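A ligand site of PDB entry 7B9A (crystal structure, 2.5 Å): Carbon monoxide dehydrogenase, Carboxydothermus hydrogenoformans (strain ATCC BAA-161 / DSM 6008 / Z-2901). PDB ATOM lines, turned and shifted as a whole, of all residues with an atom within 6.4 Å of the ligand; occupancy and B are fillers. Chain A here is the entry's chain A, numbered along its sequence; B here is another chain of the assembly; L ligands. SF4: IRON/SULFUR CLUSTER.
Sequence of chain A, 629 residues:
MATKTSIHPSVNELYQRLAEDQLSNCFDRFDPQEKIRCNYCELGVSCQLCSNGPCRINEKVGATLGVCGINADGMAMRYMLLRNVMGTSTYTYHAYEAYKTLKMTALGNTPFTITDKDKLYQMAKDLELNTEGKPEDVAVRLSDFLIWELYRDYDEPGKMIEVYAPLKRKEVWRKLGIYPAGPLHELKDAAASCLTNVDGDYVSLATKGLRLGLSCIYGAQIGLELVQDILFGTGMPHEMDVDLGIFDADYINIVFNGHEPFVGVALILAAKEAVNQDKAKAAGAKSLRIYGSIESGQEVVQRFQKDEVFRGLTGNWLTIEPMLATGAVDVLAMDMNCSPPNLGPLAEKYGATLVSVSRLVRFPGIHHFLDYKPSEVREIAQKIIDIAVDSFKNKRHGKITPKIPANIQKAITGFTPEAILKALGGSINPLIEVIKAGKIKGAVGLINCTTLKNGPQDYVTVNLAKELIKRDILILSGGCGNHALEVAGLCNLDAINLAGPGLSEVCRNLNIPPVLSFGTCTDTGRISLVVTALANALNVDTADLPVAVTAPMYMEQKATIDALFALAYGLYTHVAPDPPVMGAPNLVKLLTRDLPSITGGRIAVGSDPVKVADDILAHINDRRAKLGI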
ATOM      1  N   CYS A  47      28.375  -3.265  10.408  1.00  0.00           N
ATOM      2  CA  CYS A  47      28.700  -2.739  11.723  1.00  0.00           C
ATOM      3  C   CYS A  47      29.642  -3.675  12.455  1.00  0.00           C
ATOM      4  O   CYS A  47      29.641  -4.891  12.229  1.00  0.00           O
ATOM      5  CB  CYS A  47      27.437  -2.492  12.551  1.00  0.00           C
ATOM      6  SG  CYS A  47      27.658  -1.241  13.834  1.00  0.00           S
ATOM      7  N   GLN A  48      30.461  -3.106  13.337  1.00  0.00           N
ATOM      8  CA  GLN A  48      31.425  -3.867  14.123  1.00  0.00           C
ATOM      9  C   GLN A  48      31.528  -3.354  15.562  1.00  0.00           C
ATOM     10  O   GLN A  48      32.574  -3.489  16.199  1.00  0.00           O
ATOM     11  CB  GLN A  48      32.823  -3.838  13.496  1.00  0.00           C
ATOM     12  CG  GLN A  48      32.900  -4.350  12.054  1.00  0.00           C
ATOM     13  CD  GLN A  48      32.566  -3.269  11.036  1.00  0.00           C
ATOM     14  OE1 GLN A  48      32.760  -2.085  11.281  1.00  0.00           O
ATOM     15  NE2 GLN A  48      32.051  -3.688   9.883  1.00  0.00           N
ATOM     16  N   LEU A  49      30.447  -2.768  16.086  1.00  0.00           N
ATOM     17  CA  LEU A  49      30.520  -2.058  17.357  1.00  0.00           C
ATOM     18  C   LEU A  49      30.297  -2.944  18.580  1.00  0.00           C
ATOM     19  O   LEU A  49      30.489  -2.465  19.704  1.00  0.00           O
ATOM     20  CB  LEU A  49      29.503  -0.909  17.386  1.00  0.00           C
ATOM     21  CG  LEU A  49      29.748   0.245  16.415  1.00  0.00           C
ATOM     22  CD1 LEU A  49      28.837   1.424  16.724  1.00  0.00           C
ATOM     23  CD2 LEU A  49      31.201   0.663  16.434  1.00  0.00           C
ATOM     24  N   CYS A  50      29.897  -4.195  18.401  1.00  0.00           N
ATOM     25  CA  CYS A  50      29.588  -5.030  19.557  1.00  0.00           C
ATOM     26  C   CYS A  50      29.807  -6.497  19.207  1.00  0.00           C
ATOM     27  O   CYS A  50      29.905  -6.882  18.046  1.00  0.00           O
ATOM     28  CB  CYS A  50      28.146  -4.787  20.040  1.00  0.00           C
ATOM     29  SG  CYS A  50      27.221  -6.286  20.418  1.00  0.00           S
ATOM     30  N   SER A  51      29.882  -7.317  20.259  1.00  0.00           N
ATOM     31  CA  SER A  51      30.202  -8.734  20.091  1.00  0.00           C
ATOM     32  C   SER A  51      29.084  -9.518  19.428  1.00  0.00           C
ATOM     33  O   SER A  51      29.356 -10.579  18.849  1.00  0.00           O
ATOM     34  CB  SER A  51      30.543  -9.369  21.449  1.00  0.00           C
ATOM     35  OG  SER A  51      29.401  -9.403  22.292  1.00  0.00           O
ATOM     36  N   ASN A  52      27.840  -9.039  19.490  1.00  0.00           N
ATOM     37  CA  ASN A  52      26.769  -9.682  18.745  1.00  0.00           C
ATOM     38  C   ASN A  52      26.994  -9.598  17.248  1.00  0.00           C
ATOM     39  O   ASN A  52      26.387 -10.371  16.488  1.00  0.00           O
ATOM     40  CB  ASN A  52      25.421  -9.048  19.109  1.00  0.00           C
ATOM     41  CG  ASN A  52      24.903  -9.521  20.455  1.00  0.00           C
ATOM     42  OD1 ASN A  52      24.795 -10.714  20.710  1.00  0.00           O
ATOM     43  ND2 ASN A  52      24.577  -8.565  21.327  1.00  0.00           N
ATOM     44  N   GLY A  53      27.846  -8.681  16.793  1.00  0.00           N
ATOM     45  CA  GLY A  53      28.211  -8.592  15.400  1.00  0.00           C
ATOM     46  C   GLY A  53      29.313  -9.558  15.040  1.00  0.00           C
ATOM     47  O   GLY A  53      29.607 -10.507  15.786  1.00  0.00           O
ATOM     48  N   PRO A  54      29.968  -9.348  13.882  1.00  0.00           N
ATOM     49  CA  PRO A  54      29.709  -8.277  12.912  1.00  0.00           C
ATOM     50  C   PRO A  54      28.375  -8.446  12.204  1.00  0.00           C
ATOM     51  O   PRO A  54      28.008  -9.565  11.846  1.00  0.00           O
ATOM     52  CB  PRO A  54      30.876  -8.406  11.923  1.00  0.00           C
ATOM     53  CG  PRO A  54      31.875  -9.279  12.600  1.00  0.00           C
ATOM     54  CD  PRO A  54      31.092 -10.194  13.465  1.00  0.00           C
ATOM     55  N   CYS A  55      27.664  -7.349  12.003  1.00  0.00           N
ATOM     56  CA  CYS A  55      26.332  -7.392  11.419  1.00  0.00           C
ATOM     57  C   CYS A  55      26.320  -6.718  10.049  1.00  0.00           C
ATOM     58  O   CYS A  55      26.996  -5.711   9.833  1.00  0.00           O
ATOM     59  CB  CYS A  55      25.302  -6.724  12.335  1.00  0.00           C
ATOM     60  SG  CYS A  55      24.686  -7.830  13.619  1.00  0.00           S
ATOM     61  N   ARG A  56      25.548  -7.297   9.142  1.00  0.00           N
ATOM     62  CA  ARG A  56      25.312  -6.744   7.820  1.00  0.00           C
ATOM     63  C   ARG A  56      23.817  -6.547   7.617  1.00  0.00           C
ATOM     64  O   ARG A  56      23.001  -7.272   8.196  1.00  0.00           O
ATOM     65  CB  ARG A  56      25.872  -7.652   6.729  1.00  0.00           C
ATOM     66  CG  ARG A  56      27.382  -7.792   6.729  1.00  0.00           C
ATOM     67  CD  ARG A  56      27.820  -8.955   5.854  1.00  0.00           C
ATOM     68  NE  ARG A  56      29.196  -8.826   5.395  1.00  0.00           N
ATOM     69  CZ  ARG A  56      29.812  -9.707   4.617  1.00  0.00           C
ATOM     70  NH1 ARG A  56      29.167 -10.784   4.202  1.00  0.00           N
ATOM     71  NH2 ARG A  56      31.064  -9.505   4.245  1.00  0.00           N
ATOM     72  N   LEU A  65      17.468  -5.752  10.328  1.00  0.00           N
ATOM     73  CA  LEU A  65      18.158  -4.979  11.350  1.00  0.00           C
ATOM     74  C   LEU A  65      19.364  -5.773  11.850  1.00  0.00           C
ATOM     75  O   LEU A  65      19.482  -6.974  11.616  1.00  0.00           O
ATOM     76  CB  LEU A  65      17.237  -4.655  12.532  1.00  0.00           C
ATOM     77  CG  LEU A  65      15.793  -4.233  12.222  1.00  0.00           C
ATOM     78  CD1 LEU A  65      14.965  -4.239  13.500  1.00  0.00           C
ATOM     79  CD2 LEU A  65      15.751  -2.870  11.562  1.00  0.00           C
ATOM     80  N   GLY A  66      20.257  -5.071  12.542  1.00  0.00           N
ATOM     81  CA  GLY A  66      21.287  -5.746  13.291  1.00  0.00           C
ATOM     82  C   GLY A  66      20.701  -6.469  14.486  1.00  0.00           C
ATOM     83  O   GLY A  66      19.515  -6.359  14.809  1.00  0.00           O
ATOM     84  N   VAL A  67      21.552  -7.245  15.164  1.00  0.00           N
ATOM     85  CA  VAL A  67      21.096  -7.987  16.341  1.00  0.00           C
ATOM     86  C   VAL A  67      20.535  -7.034  17.393  1.00  0.00           C
ATOM     87  O   VAL A  67      19.598  -7.375  18.126  1.00  0.00           O
ATOM     88  CB  VAL A  67      22.229  -8.865  16.910  1.00  0.00           C
ATOM     89  CG1 VAL A  67      21.747  -9.662  18.112  1.00  0.00           C
ATOM     90  CG2 VAL A  67      22.764  -9.791  15.836  1.00  0.00           C
ATOM     91  N   CYS A  68      21.092  -5.824  17.484  1.00  0.00           N
ATOM     92  CA  CYS A  68      20.580  -4.845  18.429  1.00  0.00           C
ATOM     93  C   CYS A  68      19.171  -4.392  18.054  1.00  0.00           C
ATOM     94  O   CYS A  68      18.297  -4.266  18.923  1.00  0.00           O
ATOM     95  CB  CYS A  68      21.513  -3.641  18.492  1.00  0.00           C
ATOM     96  SG  CYS A  68      21.442  -2.595  17.029  1.00  0.00           S
ATOM     97  N   GLY A  69      18.935  -4.141  16.773  1.00  0.00           N
ATOM     98  CA  GLY A  69      17.671  -3.600  16.299  1.00  0.00           C
ATOM     99  C   GLY A  69      17.797  -2.323  15.504  1.00  0.00           C
ATOM    100  O   GLY A  69      16.770  -1.781  15.069  1.00  0.00           O
ATOM    101  N   ILE A  70      19.003  -1.798  15.288  1.00  0.00           N
ATOM    102  CA  ILE A  70      19.176  -0.579  14.516  1.00  0.00           C
ATOM    103  C   ILE A  70      18.952  -0.871  13.043  1.00  0.00           C
ATOM    104  O   ILE A  70      19.181  -2.001  12.558  1.00  0.00           O
ATOM    105  CB  ILE A  70      20.562   0.033  14.776  1.00  0.00           C
ATOM    106  CG1 ILE A  70      20.559   1.531  14.524  1.00  0.00           C
ATOM    107  CG2 ILE A  70      21.627  -0.641  13.910  1.00  0.00           C
ATOM    108  CD1 ILE A  70      21.870   2.214  14.859  1.00  0.00           C
ATOM    109  N   MET A  75      22.726   2.865  11.363  1.00  0.00           N
ATOM    110  CA  MET A  75      24.048   2.241  11.286  1.00  0.00           C
ATOM    111  C   MET A  75      25.041   3.139  10.550  1.00  0.00           C
ATOM    112  O   MET A  75      26.111   3.471  11.081  1.00  0.00           O
ATOM    113  CB  MET A  75      23.914   0.888  10.588  1.00  0.00           C
ATOM    114  CG  MET A  75      25.208   0.107  10.441  1.00  0.00           C
ATOM    115  SD  MET A  75      24.905  -1.552   9.786  1.00  0.00           S
ATOM    116  CE  MET A  75      23.843  -2.235  11.052  1.00  0.00           C
ATOM    117  N   ARG A  78      25.628   6.564  12.397  1.00  0.00           N
ATOM    118  CA  ARG A  78      26.379   6.384  13.631  1.00  0.00           C
ATOM    119  C   ARG A  78      27.843   6.105  13.347  1.00  0.00           C
ATOM    120  O   ARG A  78      28.725   6.644  14.040  1.00  0.00           O
ATOM    121  CB  ARG A  78      25.771   5.242  14.453  1.00  0.00           C
ATOM    122  CG  ARG A  78      26.519   4.938  15.732  1.00  0.00           C
ATOM    123  CD  ARG A  78      25.857   3.835  16.526  1.00  0.00           C
ATOM    124  NE  ARG A  78      25.803   2.574  15.793  1.00  0.00           N
ATOM    125  CZ  ARG A  78      25.329   1.439  16.291  1.00  0.00           C
ATOM    126  NH1 ARG A  78      24.858   1.403  17.533  1.00  0.00           N
ATOM    127  NH2 ARG A  78      25.317   0.344  15.548  1.00  0.00           N
ATOM    128  N   LEU A 195      27.904   4.555  21.089  1.00  0.00           N
ATOM    129  CA  LEU A 195      27.982   3.240  21.732  1.00  0.00           C
ATOM    130  C   LEU A 195      26.705   2.446  21.467  1.00  0.00           C
ATOM    131  O   LEU A 195      25.640   3.004  21.205  1.00  0.00           O
ATOM    132  CB  LEU A 195      28.199   3.400  23.248  1.00  0.00           C
ATOM    133  CG  LEU A 195      28.700   2.172  24.008  1.00  0.00           C
ATOM    134  CD1 LEU A 195      30.197   1.968  23.799  1.00  0.00           C
ATOM    135  CD2 LEU A 195      28.363   2.267  25.489  1.00  0.00           C
ATOM    136  N   THR A 196      26.830   1.124  21.542  1.00  0.00           N
ATOM    137  CA  THR A 196      25.720   0.238  21.234  1.00  0.00           C
ATOM    138  C   THR A 196      24.545   0.482  22.186  1.00  0.00           C
ATOM    139  O   THR A 196      24.729   0.618  23.390  1.00  0.00           O
ATOM    140  CB  THR A 196      26.157  -1.231  21.311  1.00  0.00           C
ATOM    141  OG1 THR A 196      27.158  -1.476  20.320  1.00  0.00           O
ATOM    142  CG2 THR A 196      24.978  -2.161  21.085  1.00  0.00           C
ATOM    143  N   ASN A 197      23.344   0.544  21.612  1.00  0.00           N
ATOM    144  CA  ASN A 197      22.095   0.734  22.359  1.00  0.00           C
ATOM    145  C   ASN A 197      22.091   2.064  23.114  1.00  0.00           C
ATOM    146  O   ASN A 197      21.634   2.142  24.255  1.00  0.00           O
ATOM    147  CB  ASN A 197      21.847  -0.430  23.327  1.00  0.00           C
ATOM    148  CG  ASN A 197      21.678  -1.756  22.618  1.00  0.00           C
ATOM    149  OD1 ASN A 197      21.189  -1.813  21.484  1.00  0.00           O
ATOM    150  ND2 ASN A 197      22.087  -2.838  23.267  1.00  0.00           N
ATOM    151  N   GLN B  33      21.708 -12.866  10.875  1.00  0.00           N
ATOM    152  CA  GLN B  33      23.080 -12.372  10.814  1.00  0.00           C
ATOM    153  C   GLN B  33      24.091 -13.502  10.770  1.00  0.00           C
ATOM    154  O   GLN B  33      25.198 -13.305  10.262  1.00  0.00           O
ATOM    155  CB  GLN B  33      23.360 -11.456  12.001  1.00  0.00           C
ATOM    156  CG  GLN B  33      22.559 -10.158  12.011  1.00  0.00           C
ATOM    157  CD  GLN B  33      22.974  -9.211  10.899  1.00  0.00           C
ATOM    158  OE1 GLN B  33      24.058  -9.351  10.327  1.00  0.00           O
ATOM    159  NE2 GLN B  33      22.124  -8.244  10.606  1.00  0.00           N
ATOM    160  N   ARG B  37      27.728 -13.948   8.151  1.00  0.00           N
ATOM    161  CA  ARG B  37      28.781 -13.360   8.984  1.00  0.00           C
ATOM    162  C   ARG B  37      30.036 -13.085   8.163  1.00  0.00           C
ATOM    163  O   ARG B  37      30.484 -13.925   7.379  1.00  0.00           O
ATOM    164  CB  ARG B  37      29.110 -14.284  10.146  1.00  0.00           C
ATOM    165  CG  ARG B  37      28.044 -14.363  11.225  1.00  0.00           C
ATOM    166  CD  ARG B  37      27.887 -13.038  11.959  1.00  0.00           C
ATOM    167  NE  ARG B  37      27.015 -13.170  13.124  1.00  0.00           N
ATOM    168  CZ  ARG B  37      26.529 -12.158  13.826  1.00  0.00           C
ATOM    169  NH1 ARG B  37      25.743 -12.373  14.869  1.00  0.00           N
ATOM    170  NH2 ARG B  37      26.826 -10.904  13.473  1.00  0.00           N
ATOM    171  N   MET B 555      29.997  -7.502  25.788  1.00  0.00           N
ATOM    172  CA  MET B 555      29.224  -7.029  24.636  1.00  0.00           C
ATOM    173  C   MET B 555      29.887  -5.820  24.002  1.00  0.00           C
ATOM    174  O   MET B 555      30.308  -5.867  22.839  1.00  0.00           O
ATOM    175  CB  MET B 555      27.795  -6.693  25.053  1.00  0.00           C
ATOM    176  CG  MET B 555      26.770  -6.872  23.940  1.00  0.00           C
ATOM    177  SD  MET B 555      25.312  -5.839  24.148  1.00  0.00           S
ATOM    178  CE  MET B 555      26.022  -4.209  23.919  1.00  0.00           C
HETATM  179 FE1  SF4 L   1      25.364  -5.648  15.295  1.00  0.00          FE
HETATM  180 FE2  SF4 L   1      26.350  -4.837  17.666  1.00  0.00          FE
HETATM  181 FE3  SF4 L   1      24.059  -3.744  16.729  1.00  0.00          FE
HETATM  182 FE4  SF4 L   1      26.421  -3.160  15.541  1.00  0.00          FE
HETATM  183  S1  SF4 L   1      25.817  -2.598  17.687  1.00  0.00           S
HETATM  184  S2  SF4 L   1      24.464  -3.708  14.460  1.00  0.00           S
HETATM  185  S3  SF4 L   1      27.570  -5.149  15.739  1.00  0.00           S
HETATM  186  S4  SF4 L   1      24.362  -5.941  17.343  1.00  0.00           S
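The guanidinium group of Arg 37 of chain B is in hydrogen-bond range of the backbone carbonyl oxygen of Asn 52. The side-chain sulfur (SG) of Cys 55 lies within hydrogen-bond range of the guanidinium group (NH2) of Arg 37 of chain B, 3.7 Å away. N of Asn 52 lies within hydrogen-bond range of SG of Cys 50, 3.0 Å away. The side-chain sulfur (SG) of Cys 55 lies close to the side-chain amide oxygen (OE1) of Gln 33 of chain B, at 3.7 Å. N of Ile 70 sits at hydrogen-bond distance from SG of Cys 68. The side-chain sulfur (SG) of Cys 55 sits close to the backbone NH (N) of Val 67, 3.5 Å away. The backbone NH of Cys 47 is in hydrogen-bond range of the backbone carbonyl oxygen of Cys 55 (2.9 Å). SG of Cys 47 lies within hydrogen-bond range of NH2 of Arg 78 (3.3 Å).
A sulfur (S3) of the ligand sits close to the backbone NH of Gly 53 (3.7 Å). The side-chain hydroxyl of Thr 196 lies close to a sulfur (S1) of the ligand (3.2 Å). The guanidinium group (NH2) of Arg 78 sits close to a sulfur (S1) of the ligand, 3.7 Å away. A sulfur (S4) of the ligand lies close to the backbone NH (N) of Cys 68. N of Leu 49 sits close to S3 of the ligand (3.8 Å). S4 of the ligand sits close to N of Val 67 (3.8 Å). N of Cys 50 sits close to S3 of the ligand (3.7 Å).
Residues that only touch the ligand: Cys 55 (2.8 Å), Cys 47 (2.9 Å), Asn 52 (3.7 Å), Met 75 (3.8 Å) and Gly 66 (3.95 Å). Along chain A the residues within 4 Å of the ligand span positions 47 to 196. The nearest printed residue that does not touch the ligand is Ile 70 (4.2 Å).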
